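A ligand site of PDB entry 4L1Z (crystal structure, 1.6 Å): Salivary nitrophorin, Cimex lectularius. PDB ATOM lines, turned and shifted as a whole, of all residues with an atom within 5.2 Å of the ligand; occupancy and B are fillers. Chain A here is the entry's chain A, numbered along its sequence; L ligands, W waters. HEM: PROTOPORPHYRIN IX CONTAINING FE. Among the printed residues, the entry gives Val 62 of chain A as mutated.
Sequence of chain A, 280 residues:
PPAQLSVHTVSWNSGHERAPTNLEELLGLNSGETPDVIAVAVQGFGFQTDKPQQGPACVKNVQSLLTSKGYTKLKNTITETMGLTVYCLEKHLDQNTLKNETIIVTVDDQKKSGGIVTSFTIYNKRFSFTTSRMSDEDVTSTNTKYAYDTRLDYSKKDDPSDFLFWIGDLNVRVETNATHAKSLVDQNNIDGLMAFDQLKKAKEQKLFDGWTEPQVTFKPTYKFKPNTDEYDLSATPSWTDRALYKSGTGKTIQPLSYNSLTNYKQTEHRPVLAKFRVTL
NE2 of Gln 63 sits at hydrogen-bond distance from O2D of the ligand, at 3.0 Å. NZ of Lys 73 lies within salt-bridge range of O2D of the ligand, 3.3 Å away. OH of Tyr 87 lies within hydrogen-bond range of O1D of the ligand. SG of Cys 58 is bound to FE of the ligand.
The side-chain amide nitrogen (NE2) of Gln 63 lies close to the side-chain amino group (NZ) of Lys 73, at 3.1 Å. OD1 of Asp 50 lies within hydrogen-bond range of N of Gly 55, 2.9 Å away. The guanidinium group (NH1) of Arg 18 lies within hydrogen-bond range of the backbone carbonyl oxygen (O) of Pro 52. The side-chain sulfur (SG) of Cys 58 sits close to the side-chain amide nitrogen (NE2) of Gln 54 (3.4 Å). The backbone NH (N) of Thr 85 sits at hydrogen-bond distance from the backbone carbonyl oxygen (O) of Val 40 (2.9 Å). OG1 of Thr 85 lies within hydrogen-bond range of ND2 of Asn 76 (2.8 Å). The backbone NH (N) of Gln 54 lies within hydrogen-bond range of the side-chain carboxylate (OD2) of Asp 50 (2.9 Å). NH2 of Arg 18 is in hydrogen-bond range of OE1 of Gln 54 (2.7 Å).
Merely in contact with the ligand: Ser 14 (3.7 Å), His 16 (3.7 Å), Glu 17 (3.3 Å), Arg 18 (3.9 Å), Ala 19 (3.6 Å), Leu 26 (3.5 Å), Val 42 (3.8 Å), Phe 47 (3.4 Å), Asp 50 (3.4 Å), Gln 54 (3.6 Å), Gly 55 (3.5 Å), Val 59 (3.5 Å), Val 62 (3.9 Å), Asn 76 (3.5 Å), Ile 78 (3.4 Å) and Thr 85 (3.6 Å). Within 4 Å of the ligand: Ser 14, His 16, Glu 17, Arg 18, Ala 19, Leu 26, Val 42, Phe 47, Asp 50, Gln 54, Gly 55, Cys 58, Val 59, Val 62, Gln 63, Lys 73, Asn 76, Ile 78, Thr 85 and Tyr 87. The nearest printed residue that does not touch the ligand is Gly 46 (4.1 Å).
Water W1 lies within hydrogen-bond range of O1A of the ligand (2.7 Å), NZ of Lys 73 (2.9 Å) and OD1 of Asn 76 (3.4 Å). Water W2 bridges an oxygen (O1D) of the ligand and the side-chain amide oxygen of Gln 63.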
ATOM      1  N   TRP A  12      -6.119   4.651  19.869  1.00  0.00           N
ATOM      2  CA  TRP A  12      -6.546   5.756  20.718  1.00  0.00           C
ATOM      3  C   TRP A  12      -7.805   5.427  21.471  1.00  0.00           C
ATOM      4  O   TRP A  12      -8.840   5.111  20.881  1.00  0.00           O
ATOM      5  CB  TRP A  12      -6.717   6.985  19.808  1.00  0.00           C
ATOM      6  CG  TRP A  12      -6.738   8.320  20.462  1.00  0.00           C
ATOM      7  CD1 TRP A  12      -6.704   8.637  21.797  1.00  0.00           C
ATOM      8  CD2 TRP A  12      -6.870   9.566  19.765  1.00  0.00           C
ATOM      9  NE1 TRP A  12      -6.765  10.039  21.972  1.00  0.00           N
ATOM     10  CE2 TRP A  12      -6.897  10.608  20.732  1.00  0.00           C
ATOM     11  CE3 TRP A  12      -6.965   9.901  18.406  1.00  0.00           C
ATOM     12  CZ2 TRP A  12      -6.985  11.959  20.371  1.00  0.00           C
ATOM     13  CZ3 TRP A  12      -7.073  11.225  18.061  1.00  0.00           C
ATOM     14  CH2 TRP A  12      -7.070  12.237  19.030  1.00  0.00           C
ATOM     15  N   SER A  14     -10.395   7.160  22.451  1.00  0.00           N
ATOM     16  CA  SER A  14     -10.761   8.509  22.019  1.00  0.00           C
ATOM     17  C   SER A  14     -12.099   8.923  22.552  1.00  0.00           C
ATOM     18  O   SER A  14     -12.465  10.120  22.430  1.00  0.00           O
ATOM     19  CB  SER A  14     -10.753   8.553  20.486  1.00  0.00           C
ATOM     20  OG  SER A  14     -11.618   7.548  20.039  1.00  0.00           O
ATOM     21  N   GLY A  15     -12.859   8.027  23.169  1.00  0.00           N
ATOM     22  CA  GLY A  15     -14.128   8.433  23.810  1.00  0.00           C
ATOM     23  C   GLY A  15     -15.193   8.889  22.816  1.00  0.00           C
ATOM     24  O   GLY A  15     -15.581   8.120  21.917  1.00  0.00           O
ATOM     25  N   HIS A  16     -15.680  10.114  23.031  1.00  0.00           N
ATOM     26  CA  HIS A  16     -16.687  10.718  22.162  1.00  0.00           C
ATOM     27  C   HIS A  16     -16.028  11.678  21.180  1.00  0.00           C
ATOM     28  O   HIS A  16     -16.717  12.426  20.484  1.00  0.00           O
ATOM     29  CB  HIS A  16     -17.747  11.488  23.028  1.00  0.00           C
ATOM     30  CG  HIS A  16     -18.686  10.616  23.803  1.00  0.00           C
ATOM     31  ND1 HIS A  16     -19.976  10.340  23.384  1.00  0.00           N
ATOM     32  CD2 HIS A  16     -18.549   9.992  24.996  1.00  0.00           C
ATOM     33  CE1 HIS A  16     -20.590   9.585  24.280  1.00  0.00           C
ATOM     34  NE2 HIS A  16     -19.741   9.354  25.277  1.00  0.00           N
ATOM     35  N   GLU A  17     -14.732  11.652  21.042  1.00  0.00           N
ATOM     36  CA  GLU A  17     -14.011  12.628  20.233  1.00  0.00           C
ATOM     37  C   GLU A  17     -14.047  12.243  18.735  1.00  0.00           C
ATOM     38  O   GLU A  17     -13.798  11.089  18.388  1.00  0.00           O
ATOM     39  CB  GLU A  17     -12.592  12.690  20.745  1.00  0.00           C
ATOM     40  CG  GLU A  17     -11.737  13.731  20.080  1.00  0.00           C
ATOM     41  CD  GLU A  17     -12.104  15.165  20.447  1.00  0.00           C
ATOM     42  OE1 GLU A  17     -11.586  16.020  19.696  1.00  0.00           O
ATOM     43  OE2 GLU A  17     -12.819  15.422  21.483  1.00  0.00           O
ATOM     44  N   ARG A  18     -14.333  13.208  17.848  1.00  0.00           N
ATOM     45  CA  ARG A  18     -14.229  12.958  16.406  1.00  0.00           C
ATOM     46  C   ARG A  18     -12.815  12.745  15.933  1.00  0.00           C
ATOM     47  O   ARG A  18     -11.851  13.216  16.490  1.00  0.00           O
ATOM     48  CB  ARG A  18     -14.811  14.121  15.561  1.00  0.00           C
ATOM     49  CG  ARG A  18     -16.295  14.381  15.736  1.00  0.00           C
ATOM     50  CD  ARG A  18     -16.758  15.686  15.088  1.00  0.00           C
ATOM     51  NE  ARG A  18     -18.172  15.920  15.384  1.00  0.00           N
ATOM     52  CZ  ARG A  18     -19.179  15.355  14.722  1.00  0.00           C
ATOM     53  NH1 ARG A  18     -20.444  15.596  15.080  1.00  0.00           N
ATOM     54  NH2 ARG A  18     -18.941  14.541  13.706  1.00  0.00           N
ATOM     55  N   ALA A  19     -12.686  12.055  14.798  1.00  0.00           N
ATOM     56  CA  ALA A  19     -11.423  11.965  14.143  1.00  0.00           C
ATOM     57  C   ALA A  19     -10.772  13.320  13.904  1.00  0.00           C
ATOM     58  O   ALA A  19     -11.448  14.280  13.532  1.00  0.00           O
ATOM     59  CB  ALA A  19     -11.595  11.205  12.815  1.00  0.00           C
ATOM     60  N   PRO A  20      -9.459  13.423  14.120  1.00  0.00           N
ATOM     61  CA  PRO A  20      -8.768  14.646  13.755  1.00  0.00           C
ATOM     62  C   PRO A  20      -8.699  14.739  12.241  1.00  0.00           C
ATOM     63  O   PRO A  20      -8.791  13.734  11.562  1.00  0.00           O
ATOM     64  CB  PRO A  20      -7.354  14.452  14.334  1.00  0.00           C
ATOM     65  CG  PRO A  20      -7.154  12.974  14.314  1.00  0.00           C
ATOM     66  CD  PRO A  20      -8.511  12.428  14.703  1.00  0.00           C
ATOM     67  N   LEU A  23      -4.159  13.664   9.805  1.00  0.00           N
ATOM     68  CA  LEU A  23      -3.981  12.206  10.020  1.00  0.00           C
ATOM     69  C   LEU A  23      -2.559  11.727   9.736  1.00  0.00           C
ATOM     70  O   LEU A  23      -2.179  10.602  10.072  1.00  0.00           O
ATOM     71  CB  LEU A  23      -4.962  11.471   9.127  1.00  0.00           C
ATOM     72  CG  LEU A  23      -6.389  11.864   9.362  1.00  0.00           C
ATOM     73  CD1 LEU A  23      -7.246  11.486   8.168  1.00  0.00           C
ATOM     74  CD2 LEU A  23      -6.880  11.205  10.652  1.00  0.00           C
ATOM     75  N   LEU A  26      -0.634  10.947  12.894  1.00  0.00           N
ATOM     76  CA  LEU A  26      -1.285   9.807  13.578  1.00  0.00           C
ATOM     77  C   LEU A  26      -0.875   8.463  12.980  1.00  0.00           C
ATOM     78  O   LEU A  26      -0.756   7.458  13.707  1.00  0.00           O
ATOM     79  CB  LEU A  26      -2.797   9.952  13.526  1.00  0.00           C
ATOM     80  CG  LEU A  26      -3.675   9.063  14.422  1.00  0.00           C
ATOM     81  CD1 LEU A  26      -3.591   9.540  15.868  1.00  0.00           C
ATOM     82  CD2 LEU A  26      -5.121   9.069  14.004  1.00  0.00           C
ATOM     83  N   VAL A  40      -5.362   0.865  12.403  1.00  0.00           N
ATOM     84  CA  VAL A  40      -5.843   1.921  13.270  1.00  0.00           C
ATOM     85  C   VAL A  40      -7.040   1.354  14.149  1.00  0.00           C
ATOM     86  O   VAL A  40      -8.104   0.889  13.652  1.00  0.00           O
ATOM     87  CB  VAL A  40      -6.426   3.095  12.447  1.00  0.00           C
ATOM     88  CG1 VAL A  40      -6.939   4.219  13.359  1.00  0.00           C
ATOM     89  CG2 VAL A  40      -5.392   3.620  11.459  1.00  0.00           C
ATOM     90  N   VAL A  42      -9.634   2.262  17.598  1.00  0.00           N
ATOM     91  CA  VAL A  42     -10.187   3.187  18.611  1.00  0.00           C
ATOM     92  C   VAL A  42     -11.085   2.460  19.602  1.00  0.00           C
ATOM     93  O   VAL A  42     -11.640   1.394  19.295  1.00  0.00           O
ATOM     94  CB  VAL A  42     -10.948   4.369  18.016  1.00  0.00           C
ATOM     95  CG1 VAL A  42     -10.057   5.182  17.138  1.00  0.00           C
ATOM     96  CG2 VAL A  42     -12.186   3.998  17.232  1.00  0.00           C
ATOM     97  N   PHE A  45     -17.341   5.670  22.243  1.00  0.00           N
ATOM     98  CA  PHE A  45     -18.788   5.534  22.379  1.00  0.00           C
ATOM     99  C   PHE A  45     -19.496   5.994  21.108  1.00  0.00           C
ATOM    100  O   PHE A  45     -19.224   7.067  20.622  1.00  0.00           O
ATOM    101  CB  PHE A  45     -19.284   6.347  23.577  1.00  0.00           C
ATOM    102  CG  PHE A  45     -18.770   5.842  24.905  1.00  0.00           C
ATOM    103  CD1 PHE A  45     -17.689   6.455  25.523  1.00  0.00           C
ATOM    104  CD2 PHE A  45     -19.379   4.758  25.527  1.00  0.00           C
ATOM    105  CE1 PHE A  45     -17.203   5.987  26.743  1.00  0.00           C
ATOM    106  CE2 PHE A  45     -18.913   4.281  26.751  1.00  0.00           C
ATOM    107  CZ  PHE A  45     -17.808   4.887  27.350  1.00  0.00           C
ATOM    108  N   GLY A  46     -20.370   5.151  20.557  1.00  0.00           N
ATOM    109  CA  GLY A  46     -21.297   5.608  19.502  1.00  0.00           C
ATOM    110  C   GLY A  46     -20.928   5.357  18.065  1.00  0.00           C
ATOM    111  O   GLY A  46     -21.705   5.652  17.174  1.00  0.00           O
ATOM    112  N   PHE A  47     -19.757   4.787  17.792  1.00  0.00           N
ATOM    113  CA  PHE A  47     -19.319   4.642  16.414  1.00  0.00           C
ATOM    114  C   PHE A  47     -20.367   4.071  15.425  1.00  0.00           C
ATOM    115  O   PHE A  47     -20.605   4.655  14.366  1.00  0.00           O
ATOM    116  CB  PHE A  47     -18.052   3.753  16.352  1.00  0.00           C
ATOM    117  CG  PHE A  47     -16.955   4.192  17.309  1.00  0.00           C
ATOM    118  CD1 PHE A  47     -16.549   3.388  18.365  1.00  0.00           C
ATOM    119  CD2 PHE A  47     -16.282   5.386  17.110  1.00  0.00           C
ATOM    120  CE1 PHE A  47     -15.511   3.796  19.205  1.00  0.00           C
ATOM    121  CE2 PHE A  47     -15.246   5.781  17.942  1.00  0.00           C
ATOM    122  CZ  PHE A  47     -14.887   5.011  19.010  1.00  0.00           C
ATOM    123  N   GLN A  48     -20.992   2.941  15.784  1.00  0.00           N
ATOM    124  CA  GLN A  48     -21.815   2.168  14.844  1.00  0.00           C
ATOM    125  C   GLN A  48     -23.064   2.915  14.442  1.00  0.00           C
ATOM    126  O   GLN A  48     -23.345   3.033  13.236  1.00  0.00           O
ATOM    127  CB  GLN A  48     -22.232   0.837  15.472  1.00  0.00           C
ATOM    128  CG  GLN A  48     -22.948  -0.126  14.560  1.00  0.00           C
ATOM    129  CD  GLN A  48     -23.211  -1.433  15.288  1.00  0.00           C
ATOM    130  OE1 GLN A  48     -23.463  -1.432  16.493  1.00  0.00           O
ATOM    131  NE2 GLN A  48     -23.132  -2.551  14.565  1.00  0.00           N
ATOM    132  N   ASP A  50     -23.579   6.111  15.091  1.00  0.00           N
ATOM    133  CA  ASP A  50     -23.022   7.303  14.499  1.00  0.00           C
ATOM    134  C   ASP A  50     -24.022   8.440  14.486  1.00  0.00           C
ATOM    135  O   ASP A  50     -24.230   9.063  13.440  1.00  0.00           O
ATOM    136  CB  ASP A  50     -22.527   7.034  13.077  1.00  0.00           C
ATOM    137  CG  ASP A  50     -21.732   8.171  12.532  1.00  0.00           C
ATOM    138  OD1 ASP A  50     -21.499   8.198  11.292  1.00  0.00           O
ATOM    139  OD2 ASP A  50     -21.346   9.061  13.347  1.00  0.00           O
ATOM    140  N   PRO A  52     -23.519  11.399  15.732  1.00  0.00           N
ATOM    141  CA  PRO A  52     -22.764  12.611  15.310  1.00  0.00           C
ATOM    142  C   PRO A  52     -22.516  12.767  13.788  1.00  0.00           C
ATOM    143  O   PRO A  52     -21.920  13.780  13.366  1.00  0.00           O
ATOM    144  CB  PRO A  52     -21.400  12.444  16.006  1.00  0.00           C
ATOM    145  CG  PRO A  52     -21.644  11.475  17.125  1.00  0.00           C
ATOM    146  CD  PRO A  52     -22.696  10.533  16.608  1.00  0.00           C
ATOM    147  N   GLN A  54     -20.341  11.386  11.859  1.00  0.00           N
ATOM    148  CA  GLN A  54     -18.924  11.539  11.657  1.00  0.00           C
ATOM    149  C   GLN A  54     -18.380  10.603  10.598  1.00  0.00           C
ATOM    150  O   GLN A  54     -17.376  10.903  10.004  1.00  0.00           O
ATOM    151  CB  GLN A  54     -18.210  11.274  13.006  1.00  0.00           C
ATOM    152  CG  GLN A  54     -16.714  11.139  12.950  1.00  0.00           C
ATOM    153  CD  GLN A  54     -16.063  12.409  12.561  1.00  0.00           C
ATOM    154  OE1 GLN A  54     -16.629  13.471  12.761  1.00  0.00           O
ATOM    155  NE2 GLN A  54     -14.898  12.327  12.009  1.00  0.00           N
ATOM    156  N   GLY A  55     -18.962   9.413  10.459  1.00  0.00           N
ATOM    157  CA  GLY A  55     -18.522   8.448   9.435  1.00  0.00           C
ATOM    158  C   GLY A  55     -17.987   8.981   8.106  1.00  0.00           C
ATOM    159  O   GLY A  55     -16.903   8.642   7.646  1.00  0.00           O
ATOM    160  N   CYS A  58     -14.600  10.687   8.309  1.00  0.00           N
ATOM    161  CA  CYS A  58     -13.532   9.722   8.559  1.00  0.00           C
ATOM    162  C   CYS A  58     -13.168   9.119   7.224  1.00  0.00           C
ATOM    163  O   CYS A  58     -12.018   9.156   6.814  1.00  0.00           O
ATOM    164  CB  CYS A  58     -13.969   8.593   9.521  1.00  0.00           C
ATOM    165  SG  CYS A  58     -14.343   9.105  11.205  1.00  0.00           S
ATOM    166  N   VAL A  59     -14.173   8.604   6.530  1.00  0.00           N
ATOM    167  CA  VAL A  59     -13.977   7.969   5.207  1.00  0.00           C
ATOM    168  C   VAL A  59     -13.378   8.977   4.228  1.00  0.00           C
ATOM    169  O   VAL A  59     -12.269   8.807   3.748  1.00  0.00           O
ATOM    170  CB  VAL A  59     -15.283   7.330   4.652  1.00  0.00           C
ATOM    171  CG1 VAL A  59     -15.097   6.751   3.254  1.00  0.00           C
ATOM    172  CG2 VAL A  59     -15.792   6.188   5.547  1.00  0.00           C
ATOM    173  N   VAL A  62      -9.683   9.945   5.317  1.00  0.00           N
ATOM    174  CA  VAL A  62      -8.686   8.877   5.221  1.00  0.00           C
ATOM    175  C   VAL A  62      -8.619   8.406   3.765  1.00  0.00           C
ATOM    176  O   VAL A  62      -7.509   8.310   3.205  1.00  0.00           O
ATOM    177  CB  VAL A  62      -8.963   7.602   6.078  1.00  0.00           C
ATOM    178  CG1 VAL A  62      -7.781   6.648   5.914  1.00  0.00           C
ATOM    179  CG2 VAL A  62      -9.139   7.950   7.554  1.00  0.00           C
ATOM    180  N   GLN A  63      -9.803   8.096   3.193  1.00  0.00           N
ATOM    181  CA  GLN A  63      -9.862   7.424   1.856  1.00  0.00           C
ATOM    182  C   GLN A  63      -9.203   8.365   0.901  1.00  0.00           C
ATOM    183  O   GLN A  63      -8.424   7.954   0.069  1.00  0.00           O
ATOM    184  CB  GLN A  63     -11.289   6.978   1.407  1.00  0.00           C
ATOM    185  CG  GLN A  63     -11.935   5.902   2.318  1.00  0.00           C
ATOM    186  CD  GLN A  63     -12.542   4.651   1.606  1.00  0.00           C
ATOM    187  OE1 GLN A  63     -12.322   4.405   0.408  1.00  0.00           O
ATOM    188  NE2 GLN A  63     -13.294   3.848   2.374  1.00  0.00           N
ATOM    189  N   LYS A  73      -7.947  -0.502   1.513  1.00  0.00           N
ATOM    190  CA  LYS A  73      -8.590  -0.856   2.806  1.00  0.00           C
ATOM    191  C   LYS A  73      -9.058  -2.307   2.719  1.00  0.00           C
ATOM    192  O   LYS A  73      -9.932  -2.685   1.894  1.00  0.00           O
ATOM    193  CB  LYS A  73      -9.743   0.043   3.092  1.00  0.00           C
ATOM    194  CG  LYS A  73     -10.573  -0.318   4.304  1.00  0.00           C
ATOM    195  CD  LYS A  73     -11.620   0.702   4.597  1.00  0.00           C
ATOM    196  CE  LYS A  73     -12.739   0.667   3.567  1.00  0.00           C
ATOM    197  NZ  LYS A  73     -13.995   1.283   4.047  1.00  0.00           N
ATOM    198  N   ASN A  76     -12.792  -2.263   7.489  1.00  0.00           N
ATOM    199  CA  ASN A  76     -13.179  -1.389   8.619  1.00  0.00           C
ATOM    200  C   ASN A  76     -14.269  -2.124   9.349  1.00  0.00           C
ATOM    201  O   ASN A  76     -15.218  -2.594   8.716  1.00  0.00           O
ATOM    202  CB  ASN A  76     -13.727  -0.041   8.121  1.00  0.00           C
ATOM    203  CG  ASN A  76     -14.412   0.784   9.224  1.00  0.00           C
ATOM    204  OD1 ASN A  76     -15.644   0.840   9.323  1.00  0.00           O
ATOM    205  ND2 ASN A  76     -13.605   1.431  10.074  1.00  0.00           N
ATOM    206  N   ILE A  78     -16.661  -1.641  12.977  1.00  0.00           N
ATOM    207  CA  ILE A  78     -17.031  -0.781  14.088  1.00  0.00           C
ATOM    208  C   ILE A  78     -18.141  -1.414  14.922  1.00  0.00           C
ATOM    209  O   ILE A  78     -18.959  -2.182  14.427  1.00  0.00           O
ATOM    210  CB  ILE A  78     -17.435   0.656  13.635  1.00  0.00           C
ATOM    211  CG1 ILE A  78     -18.598   0.631  12.636  1.00  0.00           C
ATOM    212  CG2 ILE A  78     -16.229   1.455  13.139  1.00  0.00           C
ATOM    213  CD1 ILE A  78     -19.049   2.036  12.225  1.00  0.00           C
ATOM    214  N   THR A  85      -9.482  -0.730  11.693  1.00  0.00           N
ATOM    215  CA  THR A  85      -9.280  -0.625  10.226  1.00  0.00           C
ATOM    216  C   THR A  85      -7.934  -1.063   9.849  1.00  0.00           C
ATOM    217  O   THR A  85      -6.948  -0.723  10.499  1.00  0.00           O
ATOM    218  CB  THR A  85      -9.542   0.819   9.728  1.00  0.00           C
ATOM    219  OG1 THR A  85     -10.792   1.258  10.259  1.00  0.00           O
ATOM    220  CG2 THR A  85      -9.601   0.822   8.241  1.00  0.00           C
ATOM    221  N   TYR A  87      -5.289  -1.441   6.482  1.00  0.00           N
ATOM    222  CA  TYR A  87      -4.878  -1.124   5.121  1.00  0.00           C
ATOM    223  C   TYR A  87      -3.582  -1.806   4.691  1.00  0.00           C
ATOM    224  O   TYR A  87      -2.628  -1.987   5.477  1.00  0.00           O
ATOM    225  CB  TYR A  87      -4.648   0.422   4.971  1.00  0.00           C
ATOM    226  CG  TYR A  87      -5.713   1.298   5.480  1.00  0.00           C
ATOM    227  CD1 TYR A  87      -5.720   1.772   6.836  1.00  0.00           C
ATOM    228  CD2 TYR A  87      -6.737   1.704   4.673  1.00  0.00           C
ATOM    229  CE1 TYR A  87      -6.717   2.603   7.300  1.00  0.00           C
ATOM    230  CE2 TYR A  87      -7.732   2.517   5.136  1.00  0.00           C
ATOM    231  CZ  TYR A  87      -7.729   3.008   6.431  1.00  0.00           C
ATOM    232  OH  TYR A  87      -8.833   3.793   6.807  1.00  0.00           O
HETATM  233  CHA HEM L   1     -14.645   5.192   9.877  1.00  0.00           C
HETATM  234  CHB HEM L   1     -17.811   6.958  13.053  1.00  0.00           C
HETATM  235  CHC HEM L   1     -14.082   8.779  15.509  1.00  0.00           C
HETATM  236  CHD HEM L   1     -10.951   6.745  12.531  1.00  0.00           C
HETATM  237  C1A HEM L   1     -15.806   5.497  10.532  1.00  0.00           C
HETATM  238  C2A HEM L   1     -17.081   4.975  10.175  1.00  0.00           C
HETATM  239  C3A HEM L   1     -17.959   5.442  11.092  1.00  0.00           C
HETATM  240  C4A HEM L   1     -17.230   6.261  11.995  1.00  0.00           C
HETATM  241  CMA HEM L   1     -19.461   5.223  11.194  1.00  0.00           C
HETATM  242  CAA HEM L   1     -17.377   3.999   9.037  1.00  0.00           C
HETATM  243  CBA HEM L   1     -18.387   4.615   8.054  1.00  0.00           C
HETATM  244  CGA HEM L   1     -18.349   3.936   6.687  1.00  0.00           C
HETATM  245  O1A HEM L   1     -17.682   2.890   6.458  1.00  0.00           O
HETATM  246  O2A HEM L   1     -19.007   4.479   5.758  1.00  0.00           O
HETATM  247  C1B HEM L   1     -17.061   7.617  14.068  1.00  0.00           C
HETATM  248  C2B HEM L   1     -17.594   8.275  15.207  1.00  0.00           C
HETATM  249  C3B HEM L   1     -16.529   8.789  15.894  1.00  0.00           C
HETATM  250  C4B HEM L   1     -15.367   8.440  15.093  1.00  0.00           C
HETATM  251  CMB HEM L   1     -19.024   8.375  15.670  1.00  0.00           C
HETATM  252  CAB HEM L   1     -16.512   9.612  17.136  1.00  0.00           C
HETATM  253  CBB HEM L   1     -17.580  10.183  17.658  1.00  0.00           C
HETATM  254  C1C HEM L   1     -12.902   8.371  14.970  1.00  0.00           C
HETATM  255  C2C HEM L   1     -11.617   8.540  15.502  1.00  0.00           C
HETATM  256  C3C HEM L   1     -10.732   7.995  14.645  1.00  0.00           C
HETATM  257  C4C HEM L   1     -11.486   7.408  13.592  1.00  0.00           C
HETATM  258  CMC HEM L   1     -11.222   9.302  16.752  1.00  0.00           C
HETATM  259  CAC HEM L   1      -9.290   8.062  14.804  1.00  0.00           C
HETATM  260  CBC HEM L   1      -8.486   8.005  13.765  1.00  0.00           C
HETATM  261  C1D HEM L   1     -11.779   6.142  11.575  1.00  0.00           C
HETATM  262  C2D HEM L   1     -11.169   5.374  10.501  1.00  0.00           C
HETATM  263  C3D HEM L   1     -12.206   4.933   9.745  1.00  0.00           C
HETATM  264  C4D HEM L   1     -13.409   5.470  10.411  1.00  0.00           C
HETATM  265  CMD HEM L   1      -9.743   5.113  10.205  1.00  0.00           C
HETATM  266  CAD HEM L   1     -12.115   4.112   8.445  1.00  0.00           C
HETATM  267  CBD HEM L   1     -11.988   5.132   7.250  1.00  0.00           C
HETATM  268  CGD HEM L   1     -11.940   4.472   5.878  1.00  0.00           C
HETATM  269  O1D HEM L   1     -10.848   4.313   5.361  1.00  0.00           O
HETATM  270  O2D HEM L   1     -12.969   4.134   5.294  1.00  0.00           O
HETATM  271  NA  HEM L   1     -15.958   6.393  11.565  1.00  0.00           N
HETATM  272  NB  HEM L   1     -15.755   7.846  13.985  1.00  0.00           N
HETATM  273  NC  HEM L   1     -12.805   7.737  13.799  1.00  0.00           N
HETATM  274  ND  HEM L   1     -13.137   6.349  11.433  1.00  0.00           N
HETATM  275 FE   HEM L   1     -14.408   7.071  12.612  1.00  0.00          FE
HETATM  276  O   HOH W   1     -14.980   2.538   6.509  1.00  0.00           O
HETATM  277  O   HOH W   2     -10.012   3.731   2.594  1.00  0.00           O
